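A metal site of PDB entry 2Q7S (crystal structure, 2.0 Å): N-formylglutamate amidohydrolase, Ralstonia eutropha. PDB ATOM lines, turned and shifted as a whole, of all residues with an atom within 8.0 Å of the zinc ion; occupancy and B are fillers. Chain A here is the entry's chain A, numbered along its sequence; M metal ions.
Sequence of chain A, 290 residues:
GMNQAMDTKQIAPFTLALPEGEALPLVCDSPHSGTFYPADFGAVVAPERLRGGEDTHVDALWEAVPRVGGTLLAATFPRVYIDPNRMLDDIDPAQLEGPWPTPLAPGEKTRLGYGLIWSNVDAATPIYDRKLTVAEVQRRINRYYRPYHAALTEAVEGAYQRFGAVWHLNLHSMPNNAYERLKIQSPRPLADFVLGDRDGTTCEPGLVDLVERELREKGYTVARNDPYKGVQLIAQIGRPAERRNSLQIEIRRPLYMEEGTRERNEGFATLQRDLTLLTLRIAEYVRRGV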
ATOM      1  N   SER A  30      10.033 -10.275  20.813  1.00  0.00           N
ATOM      2  CA  SER A  30       9.662 -11.692  20.882  1.00  0.00           C
ATOM      3  C   SER A  30      10.270 -12.308  19.580  1.00  0.00           C
ATOM      4  O   SER A  30       9.594 -12.401  18.510  1.00  0.00           O
ATOM      5  CB  SER A  30       8.146 -11.843  20.984  1.00  0.00           C
ATOM      6  OG  SER A  30       7.648 -13.178  20.957  1.00  0.00           O
ATOM      7  N   PRO A  31      11.509 -12.808  19.676  1.00  0.00           N
ATOM      8  CA  PRO A  31      12.183 -13.363  18.469  1.00  0.00           C
ATOM      9  C   PRO A  31      11.729 -14.771  18.026  1.00  0.00           C
ATOM     10  O   PRO A  31      12.068 -15.203  16.938  1.00  0.00           O
ATOM     11  CB  PRO A  31      13.649 -13.419  18.888  1.00  0.00           C
ATOM     12  CG  PRO A  31      13.605 -13.544  20.372  1.00  0.00           C
ATOM     13  CD  PRO A  31      12.394 -12.819  20.867  1.00  0.00           C
ATOM     14  N   HIS A  32      11.056 -15.482  18.907  1.00  0.00           N
ATOM     15  CA  HIS A  32      10.793 -16.885  18.766  1.00  0.00           C
ATOM     16  C   HIS A  32       9.376 -17.290  18.569  1.00  0.00           C
ATOM     17  O   HIS A  32       9.115 -18.475  18.471  1.00  0.00           O
ATOM     18  CB  HIS A  32      11.384 -17.575  19.969  1.00  0.00           C
ATOM     19  CG  HIS A  32      12.864 -17.534  19.982  1.00  0.00           C
ATOM     20  ND1 HIS A  32      13.613 -17.802  21.098  1.00  0.00           N
ATOM     21  CD2 HIS A  32      13.759 -17.244  18.992  1.00  0.00           C
ATOM     22  CE1 HIS A  32      14.894 -17.693  20.809  1.00  0.00           C
ATOM     23  NE2 HIS A  32      15.019 -17.369  19.535  1.00  0.00           N
ATOM     24  N   SER A  33       8.466 -16.309  18.497  1.00  0.00           N
ATOM     25  CA  SER A  33       7.040 -16.533  18.437  1.00  0.00           C
ATOM     26  C   SER A  33       6.477 -16.708  17.023  1.00  0.00           C
ATOM     27  O   SER A  33       5.277 -16.947  16.879  1.00  0.00           O
ATOM     28  CB  SER A  33       6.264 -15.459  19.184  1.00  0.00           C
ATOM     29  OG  SER A  33       6.600 -14.134  18.793  1.00  0.00           O
ATOM     30  N   GLY A  53      10.405 -25.973  18.902  1.00  0.00           N
ATOM     31  CA  GLY A  53      11.235 -24.786  19.228  1.00  0.00           C
ATOM     32  C   GLY A  53      10.575 -23.401  19.168  1.00  0.00           C
ATOM     33  O   GLY A  53      11.258 -22.365  19.327  1.00  0.00           O
ATOM     34  N   GLU A  54       9.269 -23.360  18.894  1.00  0.00           N
ATOM     35  CA  GLU A  54       8.528 -22.135  18.926  1.00  0.00           C
ATOM     36  C   GLU A  54       8.264 -21.701  20.356  1.00  0.00           C
ATOM     37  O   GLU A  54       7.773 -22.484  21.167  1.00  0.00           O
ATOM     38  CB  GLU A  54       7.144 -22.294  18.310  1.00  0.00           C
ATOM     39  CG  GLU A  54       7.035 -22.639  16.913  1.00  0.00           C
ATOM     40  CD  GLU A  54       5.584 -22.787  16.499  1.00  0.00           C
ATOM     41  OE1 GLU A  54       4.664 -22.625  17.348  1.00  0.00           O
ATOM     42  OE2 GLU A  54       5.375 -23.054  15.316  1.00  0.00           O
ATOM     43  N   ASP A  55       8.553 -20.455  20.647  1.00  0.00           N
ATOM     44  CA  ASP A  55       7.992 -19.782  21.804  1.00  0.00           C
ATOM     45  C   ASP A  55       6.586 -19.206  21.481  1.00  0.00           C
ATOM     46  O   ASP A  55       6.385 -17.987  21.480  1.00  0.00           O
ATOM     47  CB  ASP A  55       8.873 -18.638  22.240  1.00  0.00           C
ATOM     48  CG  ASP A  55      10.242 -19.057  22.590  1.00  0.00           C
ATOM     49  OD1 ASP A  55      10.650 -20.220  22.275  1.00  0.00           O
ATOM     50  OD2 ASP A  55      10.919 -18.155  23.106  1.00  0.00           O
ATOM     51  N   THR A  56       5.657 -20.124  21.248  1.00  0.00           N
ATOM     52  CA  THR A  56       4.318 -19.785  20.716  1.00  0.00           C
ATOM     53  C   THR A  56       3.540 -18.856  21.662  1.00  0.00           C
ATOM     54  O   THR A  56       3.606 -18.981  22.907  1.00  0.00           O
ATOM     55  CB  THR A  56       3.495 -21.086  20.431  1.00  0.00           C
ATOM     56  OG1 THR A  56       4.398 -22.092  19.987  1.00  0.00           O
ATOM     57  CG2 THR A  56       2.389 -20.882  19.386  1.00  0.00           C
ATOM     58  N   VAL A  58       3.985 -15.906  22.679  1.00  0.00           N
ATOM     59  CA  VAL A  58       4.717 -15.012  23.629  1.00  0.00           C
ATOM     60  C   VAL A  58       4.489 -13.568  23.316  1.00  0.00           C
ATOM     61  O   VAL A  58       4.339 -12.720  24.200  1.00  0.00           O
ATOM     62  CB  VAL A  58       6.246 -15.319  23.670  1.00  0.00           C
ATOM     63  CG1 VAL A  58       7.002 -14.166  24.272  1.00  0.00           C
ATOM     64  CG2 VAL A  58       6.447 -16.585  24.494  1.00  0.00           C
ATOM     65  N   ARG A  79      11.809 -19.466  14.414  1.00  0.00           N
ATOM     66  CA  ARG A  79      13.183 -19.449  14.885  1.00  0.00           C
ATOM     67  C   ARG A  79      13.992 -20.670  14.447  1.00  0.00           C
ATOM     68  O   ARG A  79      15.231 -20.572  14.415  1.00  0.00           O
ATOM     69  CB  ARG A  79      13.257 -19.271  16.400  1.00  0.00           C
ATOM     70  CG  ARG A  79      12.785 -20.414  17.210  1.00  0.00           C
ATOM     71  CD  ARG A  79      13.875 -21.370  17.563  1.00  0.00           C
ATOM     72  NE  ARG A  79      14.837 -20.920  18.548  1.00  0.00           N
ATOM     73  CZ  ARG A  79      14.802 -21.149  19.859  1.00  0.00           C
ATOM     74  NH1 ARG A  79      13.795 -21.786  20.430  1.00  0.00           N
ATOM     75  NH2 ARG A  79      15.791 -20.714  20.620  1.00  0.00           N
ATOM     76  N   ASP A  83      17.160 -18.024  13.558  1.00  0.00           N
ATOM     77  CA  ASP A  83      16.929 -17.612  14.945  1.00  0.00           C
ATOM     78  C   ASP A  83      17.490 -16.215  15.144  1.00  0.00           C
ATOM     79  O   ASP A  83      18.710 -16.089  15.263  1.00  0.00           O
ATOM     80  CB  ASP A  83      17.647 -18.553  15.882  1.00  0.00           C
ATOM     81  CG  ASP A  83      17.347 -18.287  17.322  1.00  0.00           C
ATOM     82  OD1 ASP A  83      16.902 -17.156  17.660  1.00  0.00           O
ATOM     83  OD2 ASP A  83      17.523 -19.223  18.127  1.00  0.00           O
ATOM     84  N   ASN A  85      17.807 -14.449  17.738  1.00  0.00           N
ATOM     85  CA  ASN A  85      18.504 -14.274  19.013  1.00  0.00           C
ATOM     86  C   ASN A  85      19.874 -14.839  18.979  1.00  0.00           C
ATOM     87  O   ASN A  85      20.520 -14.979  20.022  1.00  0.00           O
ATOM     88  CB  ASN A  85      17.732 -14.919  20.191  1.00  0.00           C
ATOM     89  CG  ASN A  85      17.323 -13.895  21.227  1.00  0.00           C
ATOM     90  OD1 ASN A  85      17.190 -12.713  20.916  1.00  0.00           O
ATOM     91  ND2 ASN A  85      17.245 -14.326  22.464  1.00  0.00           N
ATOM     92  N   ARG A  86      20.325 -15.273  17.808  1.00  0.00           N
ATOM     93  CA  ARG A  86      21.711 -15.735  17.706  1.00  0.00           C
ATOM     94  C   ARG A  86      22.446 -14.693  16.918  1.00  0.00           C
ATOM     95  O   ARG A  86      21.837 -13.923  16.173  1.00  0.00           O
ATOM     96  CB  ARG A  86      21.780 -17.095  17.018  1.00  0.00           C
ATOM     97  CG  ARG A  86      21.045 -18.224  17.768  1.00  0.00           C
ATOM     98  CD  ARG A  86      21.552 -18.466  19.193  1.00  0.00           C
ATOM     99  NE  ARG A  86      20.838 -19.544  19.866  1.00  0.00           N
ATOM    100  CZ  ARG A  86      19.737 -19.430  20.620  1.00  0.00           C
ATOM    101  NH1 ARG A  86      19.121 -18.269  20.840  1.00  0.00           N
ATOM    102  NH2 ARG A  86      19.203 -20.524  21.163  1.00  0.00           N
ATOM    103  N   ASN A 170      13.820  -8.946  26.281  1.00  0.00           N
ATOM    104  CA  ASN A 170      13.904 -10.036  25.317  1.00  0.00           C
ATOM    105  C   ASN A 170      13.017 -11.203  25.837  1.00  0.00           C
ATOM    106  O   ASN A 170      13.273 -11.756  26.900  1.00  0.00           O
ATOM    107  CB  ASN A 170      15.416 -10.415  25.204  1.00  0.00           C
ATOM    108  CG  ASN A 170      15.715 -11.385  24.106  1.00  0.00           C
ATOM    109  OD1 ASN A 170      16.109 -12.525  24.363  1.00  0.00           O
ATOM    110  ND2 ASN A 170      15.546 -10.955  22.871  1.00  0.00           N
ATOM    111  N   LEU A 171      11.957 -11.550  25.099  1.00  0.00           N
ATOM    112  CA  LEU A 171      10.859 -12.279  25.643  1.00  0.00           C
ATOM    113  C   LEU A 171      10.810 -13.695  25.087  1.00  0.00           C
ATOM    114  O   LEU A 171      10.852 -13.872  23.872  1.00  0.00           O
ATOM    115  CB  LEU A 171       9.525 -11.536  25.290  1.00  0.00           C
ATOM    116  CG  LEU A 171       9.442 -10.068  25.730  1.00  0.00           C
ATOM    117  CD1 LEU A 171       8.139  -9.372  25.246  1.00  0.00           C
ATOM    118  CD2 LEU A 171       9.592  -9.931  27.223  1.00  0.00           C
ATOM    119  N   HIS A 172      10.620 -14.686  25.980  1.00  0.00           N
ATOM    120  CA  HIS A 172      10.662 -16.104  25.615  1.00  0.00           C
ATOM    121  C   HIS A 172       9.699 -16.928  26.416  1.00  0.00           C
ATOM    122  O   HIS A 172       9.109 -16.468  27.406  1.00  0.00           O
ATOM    123  CB  HIS A 172      12.082 -16.687  25.855  1.00  0.00           C
ATOM    124  CG  HIS A 172      13.115 -16.012  25.047  1.00  0.00           C
ATOM    125  ND1 HIS A 172      13.547 -16.526  23.835  1.00  0.00           N
ATOM    126  CD2 HIS A 172      13.710 -14.821  25.209  1.00  0.00           C
ATOM    127  CE1 HIS A 172      14.406 -15.666  23.310  1.00  0.00           C
ATOM    128  NE2 HIS A 172      14.515 -14.631  24.119  1.00  0.00           N
ATOM    129  N   SER A 173       9.502 -18.133  25.934  1.00  0.00           N
ATOM    130  CA  SER A 173       8.983 -19.215  26.758  1.00  0.00           C
ATOM    131  C   SER A 173       9.865 -20.463  26.621  1.00  0.00           C
ATOM    132  O   SER A 173      10.541 -20.667  25.629  1.00  0.00           O
ATOM    133  CB  SER A 173       7.537 -19.530  26.366  1.00  0.00           C
ATOM    134  OG  SER A 173       7.483 -20.139  25.113  1.00  0.00           O
ATOM    135  N   MET A 174       9.741 -21.347  27.579  1.00  0.00           N
ATOM    136  CA  MET A 174      10.596 -22.490  27.657  1.00  0.00           C
ATOM    137  C   MET A 174       9.779 -23.733  28.016  1.00  0.00           C
ATOM    138  O   MET A 174       8.743 -23.642  28.728  1.00  0.00           O
ATOM    139  CB  MET A 174      11.697 -22.202  28.697  1.00  0.00           C
ATOM    140  CG  MET A 174      11.187 -21.658  29.981  1.00  0.00           C
ATOM    141  SD  MET A 174      12.570 -21.462  31.349  1.00  0.00           S
ATOM    142  CE  MET A 174      11.203 -21.150  32.674  1.00  0.00           C
ATOM    143  N   PRO A 175      10.232 -24.913  27.546  1.00  0.00           N
ATOM    144  CA  PRO A 175       9.567 -26.157  27.889  1.00  0.00           C
ATOM    145  C   PRO A 175       9.838 -26.595  29.307  1.00  0.00           C
ATOM    146  O   PRO A 175      10.805 -26.134  29.946  1.00  0.00           O
ATOM    147  CB  PRO A 175      10.176 -27.148  26.878  1.00  0.00           C
ATOM    148  CG  PRO A 175      11.496 -26.591  26.607  1.00  0.00           C
ATOM    149  CD  PRO A 175      11.372 -25.118  26.648  1.00  0.00           C
ATOM    150  N   TYR A 228      18.985 -19.977  32.138  1.00  0.00           N
ATOM    151  CA  TYR A 228      19.180 -19.000  31.086  1.00  0.00           C
ATOM    152  C   TYR A 228      19.705 -17.667  31.587  1.00  0.00           C
ATOM    153  O   TYR A 228      18.972 -16.900  32.235  1.00  0.00           O
ATOM    154  CB  TYR A 228      17.866 -18.713  30.381  1.00  0.00           C
ATOM    155  CG  TYR A 228      17.268 -19.912  29.716  1.00  0.00           C
ATOM    156  CD1 TYR A 228      17.781 -20.389  28.534  1.00  0.00           C
ATOM    157  CD2 TYR A 228      16.190 -20.573  30.274  1.00  0.00           C
ATOM    158  CE1 TYR A 228      17.230 -21.480  27.922  1.00  0.00           C
ATOM    159  CE2 TYR A 228      15.626 -21.669  29.664  1.00  0.00           C
ATOM    160  CZ  TYR A 228      16.156 -22.123  28.494  1.00  0.00           C
ATOM    161  OH  TYR A 228      15.596 -23.215  27.871  1.00  0.00           O
ATOM    162  N   GLN A 248      16.614 -10.696  29.650  1.00  0.00           N
ATOM    163  CA  GLN A 248      15.909 -11.779  28.962  1.00  0.00           C
ATOM    164  C   GLN A 248      14.886 -12.361  29.937  1.00  0.00           C
ATOM    165  O   GLN A 248      15.222 -12.631  31.082  1.00  0.00           O
ATOM    166  CB  GLN A 248      16.890 -12.843  28.514  1.00  0.00           C
ATOM    167  CG  GLN A 248      16.336 -13.850  27.556  1.00  0.00           C
ATOM    168  CD  GLN A 248      17.397 -14.666  26.844  1.00  0.00           C
ATOM    169  OE1 GLN A 248      18.404 -14.139  26.366  1.00  0.00           O
ATOM    170  NE2 GLN A 248      17.184 -15.972  26.781  1.00  0.00           N
ATOM    171  N   ILE A 249      13.638 -12.508  29.530  1.00  0.00           N
ATOM    172  CA  ILE A 249      12.589 -13.107  30.390  1.00  0.00           C
ATOM    173  C   ILE A 249      11.997 -14.362  29.763  1.00  0.00           C
ATOM    174  O   ILE A 249      11.413 -14.311  28.630  1.00  0.00           O
ATOM    175  CB  ILE A 249      11.403 -12.119  30.656  1.00  0.00           C
ATOM    176  CG1 ILE A 249      11.924 -10.785  31.234  1.00  0.00           C
ATOM    177  CG2 ILE A 249      10.374 -12.780  31.579  1.00  0.00           C
ATOM    178  CD1 ILE A 249      10.827  -9.782  31.673  1.00  0.00           C
ATOM    179  N   GLU A 250      12.063 -15.462  30.517  1.00  0.00           N
ATOM    180  CA  GLU A 250      11.595 -16.773  30.041  1.00  0.00           C
ATOM    181  C   GLU A 250      10.410 -17.287  30.858  1.00  0.00           C
ATOM    182  O   GLU A 250      10.494 -17.328  32.044  1.00  0.00           O
ATOM    183  CB  GLU A 250      12.735 -17.797  30.130  1.00  0.00           C
ATOM    184  CG  GLU A 250      13.963 -17.450  29.347  1.00  0.00           C
ATOM    185  CD  GLU A 250      14.103 -18.200  28.066  1.00  0.00           C
ATOM    186  OE1 GLU A 250      13.240 -19.058  27.765  1.00  0.00           O
ATOM    187  OE2 GLU A 250      15.071 -17.929  27.341  1.00  0.00           O
ATOM    188  N   ARG A 253       6.283 -22.750  29.717  1.00  0.00           N
ATOM    189  CA  ARG A 253       5.194 -22.926  28.757  1.00  0.00           C
ATOM    190  C   ARG A 253       3.881 -23.484  29.271  1.00  0.00           C
ATOM    191  O   ARG A 253       2.839 -23.007  28.830  1.00  0.00           O
ATOM    192  CB  ARG A 253       5.696 -23.769  27.554  1.00  0.00           C
ATOM    193  CG  ARG A 253       6.485 -22.932  26.565  1.00  0.00           C
ATOM    194  CD  ARG A 253       7.232 -23.823  25.568  1.00  0.00           C
ATOM    195  NE  ARG A 253       8.190 -23.082  24.761  1.00  0.00           N
ATOM    196  CZ  ARG A 253       9.086 -23.697  23.974  1.00  0.00           C
ATOM    197  NH1 ARG A 253       9.062 -25.001  23.884  1.00  0.00           N
ATOM    198  NH2 ARG A 253       9.934 -23.003  23.272  1.00  0.00           N
HETATM  199 ZN    ZN M   1      12.998 -18.266  23.078  1.00  0.00          ZN
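The zinc ion is bound by ND1 of His 172 (2.0 Å), OD2 of Asp 55 (2.1 Å) and ND1 of His 32 (2.1 Å).
The nearest printed residue that does not touch the zinc ion is Ser 173 (4.3 Å).
NE2 of His 172 is in hydrogen-bond range of ND2 of Asn 85.
NE2 of His 172 lies within hydrogen-bond range of OD1 of Asn 170, 2.7 Å away.
A ring nitrogen (NE2) of His 32 sits at hydrogen-bond distance from the side-chain carboxylate of Asp 83, at 2.7 Å.
OD1 of Asp 55 is in salt-bridge range of NH2 of Arg 253, at 3.0 Å.
The side-chain carboxylate (OD2) of Asp 55 sits close to the backbone NH (N) of Ser 173, at 3.2 Å.
The backbone NH (N) of His 172 lies within hydrogen-bond range of the backbone carbonyl oxygen (O) of Ile 249 (2.8 Å).
NH1 of Arg 79 is in salt-bridge range of OD1 of Asp 55 (3.97 Å).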
